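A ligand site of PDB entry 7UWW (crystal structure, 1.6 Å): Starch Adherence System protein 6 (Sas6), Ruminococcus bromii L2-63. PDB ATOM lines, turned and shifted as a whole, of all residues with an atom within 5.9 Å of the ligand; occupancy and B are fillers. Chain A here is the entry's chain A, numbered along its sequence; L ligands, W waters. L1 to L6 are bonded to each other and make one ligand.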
ATOM      1  N   TYR A  23     -23.337  15.324 -15.646  1.00  0.00           N
ATOM      2  CA  TYR A  23     -24.774  15.528 -15.528  1.00  0.00           C
ATOM      3  C   TYR A  23     -25.416  15.193 -16.866  1.00  0.00           C
ATOM      4  O   TYR A  23     -25.044  15.758 -17.904  1.00  0.00           O
ATOM      5  CB  TYR A  23     -25.058  16.972 -15.128  1.00  0.00           C
ATOM      6  CG  TYR A  23     -26.495  17.310 -15.095  1.00  0.00           C
ATOM      7  CD1 TYR A  23     -27.325  16.794 -14.108  1.00  0.00           C
ATOM      8  CD2 TYR A  23     -27.041  18.153 -16.033  1.00  0.00           C
ATOM      9  CE1 TYR A  23     -28.659  17.113 -14.065  1.00  0.00           C
ATOM     10  CE2 TYR A  23     -28.396  18.465 -16.009  1.00  0.00           C
ATOM     11  CZ  TYR A  23     -29.198  17.939 -15.026  1.00  0.00           C
ATOM     12  OH  TYR A  23     -30.530  18.256 -14.972  1.00  0.00           O
ATOM     13  N   TYR A  25     -29.124  14.737 -18.908  1.00  0.00           N
ATOM     14  CA  TYR A  25     -30.557  15.024 -18.921  1.00  0.00           C
ATOM     15  C   TYR A  25     -31.153  14.756 -20.295  1.00  0.00           C
ATOM     16  O   TYR A  25     -30.475  14.807 -21.317  1.00  0.00           O
ATOM     17  CB  TYR A  25     -30.856  16.478 -18.499  1.00  0.00           C
ATOM     18  CG  TYR A  25     -30.316  17.543 -19.438  1.00  0.00           C
ATOM     19  CD1 TYR A  25     -28.975  17.907 -19.429  1.00  0.00           C
ATOM     20  CD2 TYR A  25     -31.150  18.190 -20.329  1.00  0.00           C
ATOM     21  CE1 TYR A  25     -28.483  18.877 -20.285  1.00  0.00           C
ATOM     22  CE2 TYR A  25     -30.672  19.158 -21.174  1.00  0.00           C
ATOM     23  CZ  TYR A  25     -29.344  19.517 -21.145  1.00  0.00           C
ATOM     24  OH  TYR A  25     -28.872  20.477 -21.990  1.00  0.00           O
ATOM     25  N   GLU A  29     -32.833  11.880 -16.133  1.00  0.00           N
ATOM     26  CA  GLU A  29     -31.823  12.656 -15.444  1.00  0.00           C
ATOM     27  C   GLU A  29     -31.038  11.714 -14.535  1.00  0.00           C
ATOM     28  O   GLU A  29     -31.619  10.985 -13.734  1.00  0.00           O
ATOM     29  CB  GLU A  29     -32.446  13.792 -14.623  1.00  0.00           C
ATOM     30  CG  GLU A  29     -31.431  14.782 -14.131  1.00  0.00           C
ATOM     31  CD  GLU A  29     -32.017  15.801 -13.156  1.00  0.00           C
ATOM     32  OE1 GLU A  29     -32.645  15.380 -12.172  1.00  0.00           O
ATOM     33  OE2 GLU A  29     -31.853  17.017 -13.372  1.00  0.00           O
ATOM     34  N   TRP A  33     -28.150  18.122 -10.422  1.00  0.00           N
ATOM     35  CA  TRP A  33     -26.867  18.820 -10.489  1.00  0.00           C
ATOM     36  C   TRP A  33     -26.179  18.720  -9.137  1.00  0.00           C
ATOM     37  O   TRP A  33     -26.814  18.980  -8.100  1.00  0.00           O
ATOM     38  CB  TRP A  33     -27.078  20.269 -10.893  1.00  0.00           C
ATOM     39  CG  TRP A  33     -25.776  20.993 -11.201  1.00  0.00           C
ATOM     40  CD1 TRP A  33     -25.033  21.753 -10.343  1.00  0.00           C
ATOM     41  CD2 TRP A  33     -25.061  20.977 -12.446  1.00  0.00           C
ATOM     42  NE1 TRP A  33     -23.907  22.228 -10.982  1.00  0.00           N
ATOM     43  CE2 TRP A  33     -23.889  21.760 -12.272  1.00  0.00           C
ATOM     44  CE3 TRP A  33     -25.281  20.362 -13.697  1.00  0.00           C
ATOM     45  CZ2 TRP A  33     -22.966  21.962 -13.304  1.00  0.00           C
ATOM     46  CZ3 TRP A  33     -24.351  20.571 -14.718  1.00  0.00           C
ATOM     47  CH2 TRP A  33     -23.223  21.374 -14.519  1.00  0.00           C
ATOM     48  N   ILE A  60     -23.348  17.241 -19.571  1.00  0.00           N
ATOM     49  CA  ILE A  60     -22.556  18.372 -19.096  1.00  0.00           C
ATOM     50  C   ILE A  60     -21.561  17.881 -18.056  1.00  0.00           C
ATOM     51  O   ILE A  60     -21.955  17.235 -17.066  1.00  0.00           O
ATOM     52  CB  ILE A  60     -23.445  19.479 -18.492  1.00  0.00           C
ATOM     53  CG1 ILE A  60     -24.462  19.973 -19.520  1.00  0.00           C
ATOM     54  CG2 ILE A  60     -22.561  20.623 -17.981  1.00  0.00           C
ATOM     55  CD1 ILE A  60     -25.427  21.017 -19.000  1.00  0.00           C
ATOM     56  N   LYS A  67     -21.433  27.695  -7.217  1.00  0.00           N
ATOM     57  CA  LYS A  67     -21.250  29.086  -7.605  1.00  0.00           C
ATOM     58  C   LYS A  67     -20.638  29.842  -6.436  1.00  0.00           C
ATOM     59  O   LYS A  67     -21.045  29.682  -5.285  1.00  0.00           O
ATOM     60  CB  LYS A  67     -22.600  29.692  -8.010  1.00  0.00           C
ATOM     61  CG  LYS A  67     -22.494  30.802  -9.063  1.00  0.00           C
ATOM     62  CD  LYS A  67     -23.873  31.342  -9.484  1.00  0.00           C
ATOM     63  CE  LYS A  67     -24.728  30.276 -10.189  1.00  0.00           C
ATOM     64  NZ  LYS A  67     -25.918  30.889 -10.897  1.00  0.00           N
ATOM     65  N   LYS A  71     -17.048  26.878  -9.077  1.00  0.00           N
ATOM     66  CA  LYS A  71     -17.807  26.127 -10.074  1.00  0.00           C
ATOM     67  C   LYS A  71     -17.215  26.296 -11.469  1.00  0.00           C
ATOM     68  O   LYS A  71     -16.998  27.421 -11.933  1.00  0.00           O
ATOM     69  CB  LYS A  71     -19.267  26.588 -10.074  1.00  0.00           C
ATOM     70  CG  LYS A  71     -20.173  25.906 -11.123  1.00  0.00           C
ATOM     71  CD  LYS A  71     -21.666  26.316 -10.925  1.00  0.00           C
ATOM     72  CE  LYS A  71     -22.602  25.710 -11.972  1.00  0.00           C
ATOM     73  NZ  LYS A  71     -23.970  26.302 -11.963  1.00  0.00           N
ATOM     74  N   GLN A  73     -17.908  24.329 -15.458  1.00  0.00           N
ATOM     75  CA  GLN A  73     -18.622  23.308 -16.219  1.00  0.00           C
ATOM     76  C   GLN A  73     -18.357  23.488 -17.700  1.00  0.00           C
ATOM     77  O   GLN A  73     -17.970  24.567 -18.162  1.00  0.00           O
ATOM     78  CB  GLN A  73     -20.138  23.336 -15.975  1.00  0.00           C
ATOM     79  CG  GLN A  73     -20.850  24.500 -16.650  1.00  0.00           C
ATOM     80  CD  GLN A  73     -22.347  24.499 -16.381  1.00  0.00           C
ATOM     81  OE1 GLN A  73     -22.788  24.739 -15.249  1.00  0.00           O
ATOM     82  NE2 GLN A  73     -23.142  24.266 -17.423  1.00  0.00           N
ATOM     83  N   PRO A  75     -20.421  21.789 -21.406  1.00  0.00           N
ATOM     84  CA  PRO A  75     -20.628  23.132 -21.974  1.00  0.00           C
ATOM     85  C   PRO A  75     -21.338  24.058 -20.992  1.00  0.00           C
ATOM     86  O   PRO A  75     -21.788  23.605 -19.944  1.00  0.00           O
ATOM     87  CB  PRO A  75     -21.517  22.872 -23.215  1.00  0.00           C
ATOM     88  CG  PRO A  75     -21.424  21.368 -23.487  1.00  0.00           C
ATOM     89  CD  PRO A  75     -21.202  20.755 -22.123  1.00  0.00           C
ATOM     90  N   GLU A  76     -21.476  25.355 -21.318  1.00  0.00           N
ATOM     91  CA  GLU A  76     -22.083  26.250 -20.337  1.00  0.00           C
ATOM     92  C   GLU A  76     -23.594  26.135 -20.313  1.00  0.00           C
ATOM     93  O   GLU A  76     -24.199  26.385 -19.279  1.00  0.00           O
ATOM     94  CB  GLU A  76     -21.672  27.706 -20.592  1.00  0.00           C
ATOM     95  CG  GLU A  76     -20.207  27.986 -20.218  1.00  0.00           C
ATOM     96  CD  GLU A  76     -19.915  28.000 -18.702  1.00  0.00           C
ATOM     97  OE1 GLU A  76     -18.716  27.992 -18.325  1.00  0.00           O
ATOM     98  OE2 GLU A  76     -20.863  28.025 -17.884  1.00  0.00           O
ATOM     99  N   ALA A  77     -24.232  25.743 -21.426  1.00  0.00           N
ATOM    100  CA  ALA A  77     -25.683  25.635 -21.456  1.00  0.00           C
ATOM    101  C   ALA A  77     -26.177  24.340 -22.074  1.00  0.00           C
ATOM    102  O   ALA A  77     -26.758  23.503 -21.377  1.00  0.00           O
ATOM    103  CB  ALA A  77     -26.295  26.814 -22.217  1.00  0.00           C
ATOM    104  N   ALA A  78     -25.989  24.172 -23.371  1.00  0.00           N
ATOM    105  CA  ALA A  78     -26.536  23.029 -24.098  1.00  0.00           C
ATOM    106  C   ALA A  78     -25.588  21.841 -23.968  1.00  0.00           C
ATOM    107  O   ALA A  78     -24.437  21.900 -24.427  1.00  0.00           O
ATOM    108  CB  ALA A  78     -26.740  23.377 -25.566  1.00  0.00           C
ATOM    109  N   GLY A  79     -26.058  20.776 -23.307  1.00  0.00           N
ATOM    110  CA  GLY A  79     -25.254  19.599 -23.166  1.00  0.00           C
ATOM    111  C   GLY A  79     -24.932  18.956 -24.500  1.00  0.00           C
ATOM    112  O   GLY A  79     -25.564  19.219 -25.523  1.00  0.00           O
ATOM    113  N   PRO A 255     -33.107  25.317 -27.083  1.00  0.00           N
ATOM    114  CA  PRO A 255     -32.825  23.888 -26.884  1.00  0.00           C
ATOM    115  C   PRO A 255     -33.858  22.973 -27.518  1.00  0.00           C
ATOM    116  O   PRO A 255     -33.486  21.959 -28.113  1.00  0.00           O
ATOM    117  CB  PRO A 255     -32.806  23.747 -25.347  1.00  0.00           C
ATOM    118  CG  PRO A 255     -32.425  25.090 -24.867  1.00  0.00           C
ATOM    119  CD  PRO A 255     -33.040  26.080 -25.832  1.00  0.00           C
ATOM    120  N   GLU A 515     -34.991  33.429 -23.671  1.00  0.00           N
ATOM    121  CA  GLU A 515     -36.293  32.835 -23.367  1.00  0.00           C
ATOM    122  C   GLU A 515     -37.428  33.830 -23.548  1.00  0.00           C
ATOM    123  O   GLU A 515     -37.325  34.974 -23.102  1.00  0.00           O
ATOM    124  CB  GLU A 515     -36.290  32.303 -21.928  1.00  0.00           C
ATOM    125  CG  GLU A 515     -35.445  31.040 -21.749  1.00  0.00           C
ATOM    126  CD  GLU A 515     -35.147  30.682 -20.289  1.00  0.00           C
ATOM    127  OE1 GLU A 515     -35.661  31.365 -19.371  1.00  0.00           O
ATOM    128  OE2 GLU A 515     -34.392  29.718 -20.068  1.00  0.00           O
ATOM    129  N   PRO A 520     -40.567  29.836 -21.529  1.00  0.00           N
ATOM    130  CA  PRO A 520     -39.121  29.811 -21.747  1.00  0.00           C
ATOM    131  C   PRO A 520     -38.626  28.693 -22.657  1.00  0.00           C
ATOM    132  O   PRO A 520     -37.426  28.651 -22.950  1.00  0.00           O
ATOM    133  CB  PRO A 520     -38.564  29.657 -20.311  1.00  0.00           C
ATOM    134  CG  PRO A 520     -39.647  28.924 -19.576  1.00  0.00           C
ATOM    135  CD  PRO A 520     -40.959  29.345 -20.187  1.00  0.00           C
ATOM    136  N   SER A 521     -39.521  27.825 -23.143  1.00  0.00           N
ATOM    137  CA  SER A 521     -39.135  26.853 -24.159  1.00  0.00           C
ATOM    138  C   SER A 521     -38.981  27.461 -25.560  1.00  0.00           C
ATOM    139  O   SER A 521     -38.438  26.791 -26.448  1.00  0.00           O
ATOM    140  CB  SER A 521     -40.173  25.723 -24.202  1.00  0.00           C
ATOM    141  OG  SER A 521     -41.276  26.019 -25.046  1.00  0.00           O
HETATM  142  C1  LIG L   1     -34.911  27.925 -11.938  1.00  0.00           C
HETATM  143  C2  LIG L   1     -33.991  29.169 -11.831  1.00  0.00           C
HETATM  144  C3  LIG L   1     -32.489  28.743 -11.900  1.00  0.00           C
HETATM  145  C4  LIG L   1     -32.176  27.598 -10.942  1.00  0.00           C
HETATM  146  C5  LIG L   1     -33.251  26.515 -11.038  1.00  0.00           C
HETATM  147  C6  LIG L   1     -32.977  25.469  -9.933  1.00  0.00           C
HETATM  148  O1  LIG L   1     -34.251  30.095 -12.830  1.00  0.00           O
HETATM  149  O2  LIG L   1     -31.642  29.832 -11.656  1.00  0.00           O
HETATM  150  O3  LIG L   1     -30.846  27.086 -11.322  1.00  0.00           O
HETATM  151  O4  LIG L   1     -34.604  26.973 -10.925  1.00  0.00           O
HETATM  152  O5  LIG L   1     -32.525  24.291 -10.585  1.00  0.00           O
HETATM  153  C1  LG2 L   2     -29.984  27.228 -10.296  1.00  0.00           C
HETATM  154  C2  LG2 L   2     -28.679  27.919 -10.740  1.00  0.00           C
HETATM  155  C3  LG2 L   2     -27.995  27.138 -11.864  1.00  0.00           C
HETATM  156  C4  LG2 L   2     -27.848  25.695 -11.567  1.00  0.00           C
HETATM  157  C5  LG2 L   2     -28.998  25.070 -10.894  1.00  0.00           C
HETATM  158  C6  LG2 L   2     -28.483  23.813 -10.115  1.00  0.00           C
HETATM  159  O1  LG2 L   2     -29.008  29.209 -11.174  1.00  0.00           O
HETATM  160  O2  LG2 L   2     -26.671  27.689 -12.144  1.00  0.00           O
HETATM  161  O3  LG2 L   2     -27.669  25.131 -12.972  1.00  0.00           O
HETATM  162  O4  LG2 L   2     -29.694  25.788  -9.847  1.00  0.00           O
HETATM  163  O5  LG2 L   2     -29.487  22.837 -10.143  1.00  0.00           O
HETATM  164  C1  LG3 L   3     -36.883  25.700 -16.371  1.00  0.00           C
HETATM  165  C2  LG3 L   3     -36.965  27.231 -16.238  1.00  0.00           C
HETATM  166  C3  LG3 L   3     -35.873  27.704 -15.249  1.00  0.00           C
HETATM  167  C4  LG3 L   3     -35.928  26.944 -13.924  1.00  0.00           C
HETATM  168  C5  LG3 L   3     -35.994  25.462 -14.171  1.00  0.00           C
HETATM  169  C6  LG3 L   3     -36.383  24.774 -12.804  1.00  0.00           C
HETATM  170  O1  LG3 L   3     -36.776  27.802 -17.485  1.00  0.00           O
HETATM  171  O2  LG3 L   3     -35.985  29.082 -14.961  1.00  0.00           O
HETATM  172  O3  LG3 L   3     -34.696  27.299 -13.222  1.00  0.00           O
HETATM  173  O4  LG3 L   3     -36.947  24.990 -15.110  1.00  0.00           O
HETATM  174  O5  LG3 L   3     -35.223  24.062 -12.348  1.00  0.00           O
HETATM  175  C1  LG4 L   4     -26.913  23.915 -13.013  1.00  0.00           C
HETATM  176  C2  LG4 L   4     -26.009  23.981 -14.282  1.00  0.00           C
HETATM  177  C3  LG4 L   4     -26.908  23.898 -15.571  1.00  0.00           C
HETATM  178  C4  LG4 L   4     -27.900  22.739 -15.511  1.00  0.00           C
HETATM  179  C5  LG4 L   4     -28.620  22.766 -14.193  1.00  0.00           C
HETATM  180  C6  LG4 L   4     -29.498  21.472 -14.046  1.00  0.00           C
HETATM  181  O1  LG4 L   4     -25.267  25.158 -14.313  1.00  0.00           O
HETATM  182  O2  LG4 L   4     -26.081  23.837 -16.709  1.00  0.00           O
HETATM  183  O3  LG4 L   4     -28.850  23.005 -16.602  1.00  0.00           O
HETATM  184  O4  LG4 L   4     -27.797  22.829 -13.032  1.00  0.00           O
HETATM  185  O5  LG4 L   4     -30.466  21.704 -13.019  1.00  0.00           O
HETATM  186  C1  LG5 L   5     -33.711  22.842 -19.626  1.00  0.00           C
HETATM  187  C2  LG5 L   5     -34.402  24.043 -20.348  1.00  0.00           C
HETATM  188  C3  LG5 L   5     -34.827  25.080 -19.261  1.00  0.00           C
HETATM  189  C4  LG5 L   5     -35.595  24.403 -18.138  1.00  0.00           C
HETATM  190  C5  LG5 L   5     -34.964  23.112 -17.654  1.00  0.00           C
HETATM  191  C6  LG5 L   5     -35.924  22.355 -16.688  1.00  0.00           C
HETATM  192  O1  LG5 L   5     -33.587  24.657 -21.281  1.00  0.00           O
HETATM  193  O2  LG5 L   5     -35.565  26.120 -19.889  1.00  0.00           O
HETATM  194  O3  LG5 L   5     -35.673  25.353 -17.016  1.00  0.00           O
HETATM  195  O4  LG5 L   5     -34.651  22.239 -18.723  1.00  0.00           O
HETATM  196  O5  LG5 L   5     -37.012  21.901 -17.443  1.00  0.00           O
HETATM  197  C1  LG6 L   6     -28.846  22.045 -17.659  1.00  0.00           C
HETATM  198  C2  LG6 L   6     -28.865  22.813 -18.998  1.00  0.00           C
HETATM  199  C3  LG6 L   6     -30.221  23.500 -19.210  1.00  0.00           C
HETATM  200  C4  LG6 L   6     -31.428  22.529 -19.010  1.00  0.00           C
HETATM  201  C5  LG6 L   6     -31.225  21.757 -17.705  1.00  0.00           C
HETATM  202  C6  LG6 L   6     -32.185  20.507 -17.638  1.00  0.00           C
HETATM  203  O1  LG6 L   6     -27.797  23.741 -18.981  1.00  0.00           O
HETATM  204  O2  LG6 L   6     -30.306  24.086 -20.475  1.00  0.00           O
HETATM  205  O3  LG6 L   6     -32.603  23.345 -18.906  1.00  0.00           O
HETATM  206  O4  LG6 L   6     -29.939  21.177 -17.495  1.00  0.00           O
HETATM  207  O5  LG6 L   6     -32.405  20.132 -16.274  1.00  0.00           O
HETATM  208  O   HOH W   1     -32.856  23.515 -13.878  1.00  0.00           O
HETATM  209  O   HOH W   2     -35.159  26.941 -22.918  1.00  0.00           O
HETATM  210  O   HOH W   3     -26.397  27.668 -14.995  1.00  0.00           O
HETATM  211  O   HOH W   4     -26.156  27.119 -17.786  1.00  0.00           O
HETATM  212  O   HOH W   5     -30.313  22.139 -23.148  1.00  0.00           O
HETATM  213  O   HOH W   6     -30.448  19.465 -11.133  1.00  0.00           O
HETATM  214  O   HOH W   7     -28.425  26.601 -18.394  1.00  0.00           O
HETATM  215  O   HOH W   8     -33.516  21.823 -22.704  1.00  0.00           O
HETATM  216  O   HOH W   9     -37.788  25.342 -21.218  1.00  0.00           O
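Water W6 bridges the backbone NH of Trp 33 (2.8 Å) and an oxygen (O5) of LG4 L4 (2.9 Å).
Water W2 bridges the backbone carbonyl oxygen of Pro 520 (2.8 Å) and an oxygen (O2) of LG5 L5 (3.2 Å).
Water W5 lies within hydrogen-bond range of the side-chain hydroxyl (OH) of Tyr 25 (2.5 Å) and an oxygen (O2) of LG6 L6 (3.3 Å).
Water W4 lies within hydrogen-bond range of the backbone carbonyl oxygen (O) of Glu 76 (2.6 Å) and an oxygen (O2) of LG4 L4 (3.5 Å).
The backbone NH (N) of Gly 79 sits at hydrogen-bond distance from the side-chain hydroxyl (OH) of Tyr 25.
The side-chain amide nitrogen (NE2) of Gln 73 sits at hydrogen-bond distance from the backbone carbonyl oxygen (O) of Pro 75 (2.9 Å).
The backbone NH of Tyr 23 sits at hydrogen-bond distance from the backbone carbonyl oxygen of Ile 60.
O of Glu 76 sits at hydrogen-bond distance from NE2 of Gln 73, 3.0 Å away.
The side-chain hydroxyl (OH) of Tyr 23 lies within hydrogen-bond range of the side-chain carboxylate (OE2) of Glu 29, 2.4 Å away.
Merely in contact with the ligand: Trp 33 (3.3 Å), Lys 67 (3.5 Å), Ile 60 (3.6 Å), Tyr 25 (3.7 Å), Pro 520 (3.7 Å), Glu 515 (3.8 Å) and Pro 255 (3.8 Å).
Of the 17 residues printed, 11 come within 4 Å of the ligand.
Along chain A the residues within 4 Å of the ligand span positions 23 to 520.
The nearest printed residue that does not touch the ligand is Glu 76 (4.1 Å).
O1 of LG6 L6 lies within hydrogen-bond range of O of Ala 77 (2.6 Å).
NZ of Lys 71 is in hydrogen-bond range of O1 of LG4 L4 (2.9 Å).
The side-chain hydroxyl of Tyr 23 is in hydrogen-bond range of an oxygen (O5) of LG6 L6 (3.0 Å).
The side-chain amide oxygen (OE1) of Gln 73 is in hydrogen-bond range of an oxygen (O1) of LG4 L4 (2.7 Å).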
